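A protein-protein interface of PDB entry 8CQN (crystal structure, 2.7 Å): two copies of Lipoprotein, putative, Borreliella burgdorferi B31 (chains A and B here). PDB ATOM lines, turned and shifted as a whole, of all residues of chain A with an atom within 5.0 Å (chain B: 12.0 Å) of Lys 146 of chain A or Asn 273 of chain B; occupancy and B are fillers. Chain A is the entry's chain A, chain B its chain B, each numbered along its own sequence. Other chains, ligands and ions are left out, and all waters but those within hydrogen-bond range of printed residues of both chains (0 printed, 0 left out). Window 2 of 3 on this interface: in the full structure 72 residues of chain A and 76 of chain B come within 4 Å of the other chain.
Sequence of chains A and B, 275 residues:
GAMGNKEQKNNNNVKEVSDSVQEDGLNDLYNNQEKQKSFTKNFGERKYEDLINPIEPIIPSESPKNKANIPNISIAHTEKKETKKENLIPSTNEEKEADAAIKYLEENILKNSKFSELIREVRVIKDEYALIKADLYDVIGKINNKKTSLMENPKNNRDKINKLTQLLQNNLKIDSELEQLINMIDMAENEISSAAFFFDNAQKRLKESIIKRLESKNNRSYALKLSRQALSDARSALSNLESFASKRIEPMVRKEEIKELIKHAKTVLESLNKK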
ATOM      1  N   GLY A 141     -23.104  19.803 -16.293  1.00  0.00           N
ATOM      2  CA  GLY A 141     -23.171  21.133 -16.907  1.00  0.00           C
ATOM      3  C   GLY A 141     -21.957  21.426 -17.777  1.00  0.00           C
ATOM      4  O   GLY A 141     -22.140  21.809 -18.974  1.00  0.00           O
ATOM      5  N   LYS A 142     -20.773  21.232 -17.203  1.00  0.00           N
ATOM      6  CA  LYS A 142     -19.483  21.263 -17.931  1.00  0.00           C
ATOM      7  C   LYS A 142     -19.581  20.296 -19.126  1.00  0.00           C
ATOM      8  O   LYS A 142     -19.286  20.758 -20.249  1.00  0.00           O
ATOM      9  CB  LYS A 142     -18.337  21.011 -16.937  1.00  0.00           C
ATOM     10  CG  LYS A 142     -18.112  22.192 -16.002  1.00  0.00           C
ATOM     11  CD  LYS A 142     -17.277  22.016 -14.771  1.00  0.00           C
ATOM     12  CE  LYS A 142     -17.385  23.281 -13.922  1.00  0.00           C
ATOM     13  NZ  LYS A 142     -16.636  23.235 -12.635  1.00  0.00           N
ATOM     14  N   ILE A 143     -20.068  19.052 -18.959  1.00  0.00           N
ATOM     15  CA  ILE A 143     -20.182  18.155 -20.150  1.00  0.00           C
ATOM     16  C   ILE A 143     -21.017  18.878 -21.210  1.00  0.00           C
ATOM     17  O   ILE A 143     -20.570  18.940 -22.361  1.00  0.00           O
ATOM     18  CB  ILE A 143     -20.776  16.747 -19.916  1.00  0.00           C
ATOM     19  CG1 ILE A 143     -20.225  15.983 -18.705  1.00  0.00           C
ATOM     20  CG2 ILE A 143     -20.584  15.903 -21.161  1.00  0.00           C
ATOM     21  CD1 ILE A 143     -18.744  16.046 -18.552  1.00  0.00           C
ATOM     22  N   ASN A 144     -22.187  19.392 -20.850  1.00  0.00           N
ATOM     23  CA  ASN A 144     -23.140  19.934 -21.848  1.00  0.00           C
ATOM     24  C   ASN A 144     -22.567  21.187 -22.494  1.00  0.00           C
ATOM     25  O   ASN A 144     -22.483  21.241 -23.728  1.00  0.00           O
ATOM     26  CB  ASN A 144     -24.431  20.324 -21.167  1.00  0.00           C
ATOM     27  CG  ASN A 144     -25.513  20.562 -22.166  1.00  0.00           C
ATOM     28  OD1 ASN A 144     -25.848  19.679 -22.943  1.00  0.00           O
ATOM     29  ND2 ASN A 144     -26.038  21.742 -22.150  1.00  0.00           N
ATOM     30  N   ASN A 145     -22.042  22.109 -21.680  1.00  0.00           N
ATOM     31  CA  ASN A 145     -21.458  23.358 -22.214  1.00  0.00           C
ATOM     32  C   ASN A 145     -20.306  22.997 -23.153  1.00  0.00           C
ATOM     33  O   ASN A 145     -20.185  23.636 -24.192  1.00  0.00           O
ATOM     34  CB  ASN A 145     -21.054  24.326 -21.123  1.00  0.00           C
ATOM     35  CG  ASN A 145     -22.227  24.647 -20.252  1.00  0.00           C
ATOM     36  OD1 ASN A 145     -22.058  25.042 -19.107  1.00  0.00           O
ATOM     37  ND2 ASN A 145     -23.412  24.488 -20.797  1.00  0.00           N
ATOM     38  N   LYS A 146     -19.519  21.972 -22.881  1.00  0.00           N
ATOM     39  CA  LYS A 146     -18.393  21.722 -23.813  1.00  0.00           C
ATOM     40  C   LYS A 146     -19.025  21.227 -25.108  1.00  0.00           C
ATOM     41  O   LYS A 146     -18.717  21.791 -26.184  1.00  0.00           O
ATOM     42  CB  LYS A 146     -17.336  20.806 -23.204  1.00  0.00           C
ATOM     43  CG  LYS A 146     -16.264  20.327 -24.166  1.00  0.00           C
ATOM     44  CD  LYS A 146     -15.363  21.396 -24.713  1.00  0.00           C
ATOM     45  CE  LYS A 146     -14.452  21.985 -23.659  1.00  0.00           C
ATOM     46  NZ  LYS A 146     -13.689  23.141 -24.189  1.00  0.00           N
ATOM     47  N   LYS A 147     -19.967  20.295 -25.000  1.00  0.00           N
ATOM     48  CA  LYS A 147     -20.575  19.628 -26.177  1.00  0.00           C
ATOM     49  C   LYS A 147     -21.197  20.691 -27.072  1.00  0.00           C
ATOM     50  O   LYS A 147     -20.975  20.642 -28.325  1.00  0.00           O
ATOM     51  CB  LYS A 147     -21.679  18.664 -25.757  1.00  0.00           C
ATOM     52  CG  LYS A 147     -22.174  17.759 -26.864  1.00  0.00           C
ATOM     53  CD  LYS A 147     -23.412  16.994 -26.477  1.00  0.00           C
ATOM     54  CE  LYS A 147     -24.606  17.909 -26.370  1.00  0.00           C
ATOM     55  NZ  LYS A 147     -25.744  17.346 -27.122  1.00  0.00           N
ATOM     56  N   THR A 148     -21.936  21.623 -26.471  1.00  0.00           N
ATOM     57  CA  THR A 148     -22.615  22.652 -27.278  1.00  0.00           C
ATOM     58  C   THR A 148     -21.583  23.416 -28.121  1.00  0.00           C
ATOM     59  O   THR A 148     -21.736  23.512 -29.367  1.00  0.00           O
ATOM     60  CB  THR A 148     -23.410  23.587 -26.388  1.00  0.00           C
ATOM     61  OG1 THR A 148     -24.127  22.713 -25.517  1.00  0.00           O
ATOM     62  CG2 THR A 148     -24.307  24.494 -27.206  1.00  0.00           C
ATOM     63  N   SER A 149     -20.520  23.885 -27.491  1.00  0.00           N
ATOM     64  CA  SER A 149     -19.439  24.641 -28.170  1.00  0.00           C
ATOM     65  C   SER A 149     -18.905  23.809 -29.337  1.00  0.00           C
ATOM     66  O   SER A 149     -18.978  24.238 -30.445  1.00  0.00           O
ATOM     67  CB  SER A 149     -18.375  24.984 -27.171  1.00  0.00           C
ATOM     68  OG  SER A 149     -17.288  25.602 -27.805  1.00  0.00           O
ATOM     69  N   LEU A 150     -18.433  22.621 -29.061  1.00  0.00           N
ATOM     70  CA  LEU A 150     -17.919  21.694 -30.083  1.00  0.00           C
ATOM     71  C   LEU A 150     -18.968  21.516 -31.191  1.00  0.00           C
ATOM     72  O   LEU A 150     -18.623  21.161 -32.333  1.00  0.00           O
ATOM     73  CB  LEU A 150     -17.559  20.387 -29.366  1.00  0.00           C
ATOM     74  CG  LEU A 150     -16.072  20.090 -29.183  1.00  0.00           C
ATOM     75  CD1 LEU A 150     -15.240  21.312 -28.848  1.00  0.00           C
ATOM     76  CD2 LEU A 150     -15.859  19.017 -28.119  1.00  0.00           C
ATOM     77  N   MET A 151     -20.237  21.729 -30.911  1.00  0.00           N
ATOM     78  CA  MET A 151     -21.235  21.384 -31.948  1.00  0.00           C
ATOM     79  C   MET A 151     -21.288  22.435 -33.066  1.00  0.00           C
ATOM     80  O   MET A 151     -21.914  22.139 -34.073  1.00  0.00           O
ATOM     81  CB  MET A 151     -22.613  21.175 -31.331  1.00  0.00           C
ATOM     82  CG  MET A 151     -22.850  19.747 -31.044  1.00  0.00           C
ATOM     83  SD  MET A 151     -24.286  19.479 -29.998  1.00  0.00           S
ATOM     84  CE  MET A 151     -24.530  17.755 -30.438  1.00  0.00           C
ATOM     85  N   LEU A 164     -18.499  12.689 -25.436  1.00  0.00           N
ATOM     86  CA  LEU A 164     -19.187  13.650 -24.570  1.00  0.00           C
ATOM     87  C   LEU A 164     -20.657  13.216 -24.461  1.00  0.00           C
ATOM     88  O   LEU A 164     -21.203  13.223 -23.321  1.00  0.00           O
ATOM     89  CB  LEU A 164     -19.014  15.027 -25.218  1.00  0.00           C
ATOM     90  CG  LEU A 164     -18.189  16.080 -24.470  1.00  0.00           C
ATOM     91  CD1 LEU A 164     -16.986  15.506 -23.802  1.00  0.00           C
ATOM     92  CD2 LEU A 164     -17.750  17.193 -25.387  1.00  0.00           C
ATOM     93  N   HIS B 264     -14.110   9.803 -11.770  1.00  0.00           N
ATOM     94  CA  HIS B 264     -13.783   9.292 -13.119  1.00  0.00           C
ATOM     95  C   HIS B 264     -14.374  10.208 -14.199  1.00  0.00           C
ATOM     96  O   HIS B 264     -13.645  10.580 -15.127  1.00  0.00           O
ATOM     97  CB  HIS B 264     -14.270   7.855 -13.274  1.00  0.00           C
ATOM     98  CG  HIS B 264     -14.113   7.303 -14.647  1.00  0.00           C
ATOM     99  ND1 HIS B 264     -15.145   7.319 -15.580  1.00  0.00           N
ATOM    100  CD2 HIS B 264     -13.063   6.716 -15.257  1.00  0.00           C
ATOM    101  CE1 HIS B 264     -14.739   6.767 -16.697  1.00  0.00           C
ATOM    102  NE2 HIS B 264     -13.461   6.384 -16.524  1.00  0.00           N
ATOM    103  N   ALA B 265     -15.654  10.533 -14.121  1.00  0.00           N
ATOM    104  CA  ALA B 265     -16.307  11.353 -15.155  1.00  0.00           C
ATOM    105  C   ALA B 265     -15.470  12.616 -15.428  1.00  0.00           C
ATOM    106  O   ALA B 265     -15.281  12.971 -16.636  1.00  0.00           O
ATOM    107  CB  ALA B 265     -17.707  11.688 -14.723  1.00  0.00           C
ATOM    108  N   LYS B 266     -14.968  13.284 -14.385  1.00  0.00           N
ATOM    109  CA  LYS B 266     -14.331  14.604 -14.591  1.00  0.00           C
ATOM    110  C   LYS B 266     -12.930  14.362 -15.144  1.00  0.00           C
ATOM    111  O   LYS B 266     -12.450  15.192 -15.916  1.00  0.00           O
ATOM    112  CB  LYS B 266     -14.417  15.477 -13.344  1.00  0.00           C
ATOM    113  CG  LYS B 266     -13.621  15.018 -12.137  1.00  0.00           C
ATOM    114  CD  LYS B 266     -14.334  15.297 -10.828  1.00  0.00           C
ATOM    115  CE  LYS B 266     -14.553  16.771 -10.553  1.00  0.00           C
ATOM    116  NZ  LYS B 266     -15.397  16.968  -9.347  1.00  0.00           N
ATOM    117  N   THR B 267     -12.372  13.196 -14.856  1.00  0.00           N
ATOM    118  CA  THR B 267     -11.121  12.685 -15.452  1.00  0.00           C
ATOM    119  C   THR B 267     -11.303  12.552 -16.949  1.00  0.00           C
ATOM    120  O   THR B 267     -10.465  13.106 -17.689  1.00  0.00           O
ATOM    121  CB  THR B 267     -10.747  11.377 -14.764  1.00  0.00           C
ATOM    122  OG1 THR B 267     -10.273  11.824 -13.502  1.00  0.00           O
ATOM    123  CG2 THR B 267      -9.666  10.561 -15.430  1.00  0.00           C
ATOM    124  N   VAL B 268     -12.363  11.863 -17.387  1.00  0.00           N
ATOM    125  CA  VAL B 268     -12.647  11.699 -18.843  1.00  0.00           C
ATOM    126  C   VAL B 268     -12.674  13.087 -19.474  1.00  0.00           C
ATOM    127  O   VAL B 268     -12.048  13.258 -20.499  1.00  0.00           O
ATOM    128  CB  VAL B 268     -13.927  10.914 -19.155  1.00  0.00           C
ATOM    129  CG1 VAL B 268     -14.227  10.933 -20.642  1.00  0.00           C
ATOM    130  CG2 VAL B 268     -13.818   9.485 -18.694  1.00  0.00           C
ATOM    131  N   LEU B 269     -13.312  14.050 -18.828  1.00  0.00           N
ATOM    132  CA  LEU B 269     -13.617  15.361 -19.457  1.00  0.00           C
ATOM    133  C   LEU B 269     -12.344  16.175 -19.562  1.00  0.00           C
ATOM    134  O   LEU B 269     -12.148  16.778 -20.603  1.00  0.00           O
ATOM    135  CB  LEU B 269     -14.671  16.127 -18.635  1.00  0.00           C
ATOM    136  CG  LEU B 269     -14.888  17.576 -19.056  1.00  0.00           C
ATOM    137  CD1 LEU B 269     -15.236  17.663 -20.513  1.00  0.00           C
ATOM    138  CD2 LEU B 269     -15.951  18.234 -18.224  1.00  0.00           C
ATOM    139  N   GLU B 270     -11.551  16.243 -18.502  1.00  0.00           N
ATOM    140  CA  GLU B 270     -10.241  16.940 -18.568  1.00  0.00           C
ATOM    141  C   GLU B 270      -9.469  16.388 -19.772  1.00  0.00           C
ATOM    142  O   GLU B 270      -9.096  17.205 -20.622  1.00  0.00           O
ATOM    143  CB  GLU B 270      -9.457  16.800 -17.270  1.00  0.00           C
ATOM    144  CG  GLU B 270      -8.583  18.016 -17.008  1.00  0.00           C
ATOM    145  CD  GLU B 270      -7.465  17.788 -16.002  1.00  0.00           C
ATOM    146  OE1 GLU B 270      -7.546  16.786 -15.265  1.00  0.00           O
ATOM    147  OE2 GLU B 270      -6.515  18.606 -15.961  1.00  0.00           O
ATOM    148  N   SER B 271      -9.342  15.057 -19.874  1.00  0.00           N
ATOM    149  CA  SER B 271      -8.562  14.320 -20.900  1.00  0.00           C
ATOM    150  C   SER B 271      -8.969  14.705 -22.314  1.00  0.00           C
ATOM    151  O   SER B 271      -8.092  14.777 -23.184  1.00  0.00           O
ATOM    152  CB  SER B 271      -8.719  12.863 -20.735  1.00  0.00           C
ATOM    153  OG  SER B 271      -8.019  12.458 -19.583  1.00  0.00           O
ATOM    154  N   LEU B 272     -10.258  14.893 -22.567  1.00  0.00           N
ATOM    155  CA  LEU B 272     -10.684  15.340 -23.914  1.00  0.00           C
ATOM    156  C   LEU B 272      -9.971  16.634 -24.263  1.00  0.00           C
ATOM    157  O   LEU B 272      -9.557  16.746 -25.414  1.00  0.00           O
ATOM    158  CB  LEU B 272     -12.192  15.525 -23.952  1.00  0.00           C
ATOM    159  CG  LEU B 272     -12.942  14.210 -23.924  1.00  0.00           C
ATOM    160  CD1 LEU B 272     -14.368  14.448 -24.330  1.00  0.00           C
ATOM    161  CD2 LEU B 272     -12.303  13.171 -24.830  1.00  0.00           C
ATOM    162  N   ASN B 273      -9.775  17.521 -23.281  1.00  0.00           N
ATOM    163  CA  ASN B 273      -9.284  18.916 -23.474  1.00  0.00           C
ATOM    164  C   ASN B 273      -7.768  18.876 -23.726  1.00  0.00           C
ATOM    165  O   ASN B 273      -7.072  19.838 -23.366  1.00  0.00           O
ATOM    166  CB  ASN B 273      -9.785  19.813 -22.329  1.00  0.00           C
ATOM    167  CG  ASN B 273     -11.308  19.890 -22.264  1.00  0.00           C
ATOM    168  OD1 ASN B 273     -11.909  20.007 -21.197  1.00  0.00           O
ATOM    169  ND2 ASN B 273     -11.965  19.832 -23.409  1.00  0.00           N
ATOM    170  N   LYS B 274      -7.292  17.819 -24.401  1.00  0.00           N
ATOM    171  CA  LYS B 274      -5.864  17.546 -24.699  1.00  0.00           C
ATOM    172  C   LYS B 274      -5.759  16.720 -25.990  1.00  0.00           C
ATOM    173  O   LYS B 274      -6.572  16.729 -26.927  1.00  0.00           O
ATOM    174  CB  LYS B 274      -5.261  16.783 -23.516  1.00  0.00           C
ATOM    175  CG  LYS B 274      -5.471  17.418 -22.145  1.00  0.00           C
ATOM    176  CD  LYS B 274      -4.994  16.523 -21.036  1.00  0.00           C
ATOM    177  CE  LYS B 274      -4.767  17.218 -19.712  1.00  0.00           C
ATOM    178  NZ  LYS B 274      -4.066  16.295 -18.785  1.00  0.00           N
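Leu 269 of chain B touches Lys 142 of chain A (CD2 to CB, 3.9 Å). Ile 143 of chain A touches Leu 269 of chain B (CD1 to CD2, 3.6 Å). Asn 273 of chain B touches Lys 146 of chain A (ND2 to CE, 3.3 Å). Leu 272 of chain B touches Leu 164 of chain A (CD1 to CD1, 2.9 Å).
Lys 146 of chain A touches just one residue of chain B: Asn 273. Asn 273 of chain B touches just one residue of chain A: Lys 146 (3.3 Å). Gly 141 of chain A touches none of the printed residues of chain B. Ile 143 of chain A touches just one residue of chain B: Leu 269. No residue of chain B comes within 4 Å of Asn 144 of chain A. No residue of chain B comes within 4 Å of Asn 145 of chain A. No residue of chain B comes within 4 Å of Thr 148 of chain A. No residue of chain B comes within 4 Å of Ser 149 of chain A. Of the printed residues of chain A, Leu 272 of chain B touches Leu 164 (2.9 Å). Of the printed residues of chain B, Lys 142 of chain A touches Leu 269. Lys 274 of chain B touches none of the printed residues of chain A. The nearest printed residue of chain A that does not touch Asn 273 of chain B is Leu 150 of chain A (6.2 Å). The nearest printed residue of chain A that does not touch Leu 269 of chain B is Leu 164 of chain A (4.3 Å).
O of Leu 269 of chain B lies close to OD1 of Asn 273 of chain B, at 3.3 Å.
Of the 12 printed residues of chain A, 4 touch a printed residue of chain B. Hydrophobic or aromatic side chains of chain B that line the printed part of chain A: Leu 269 and Leu 272.
No position is printed for both chains.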
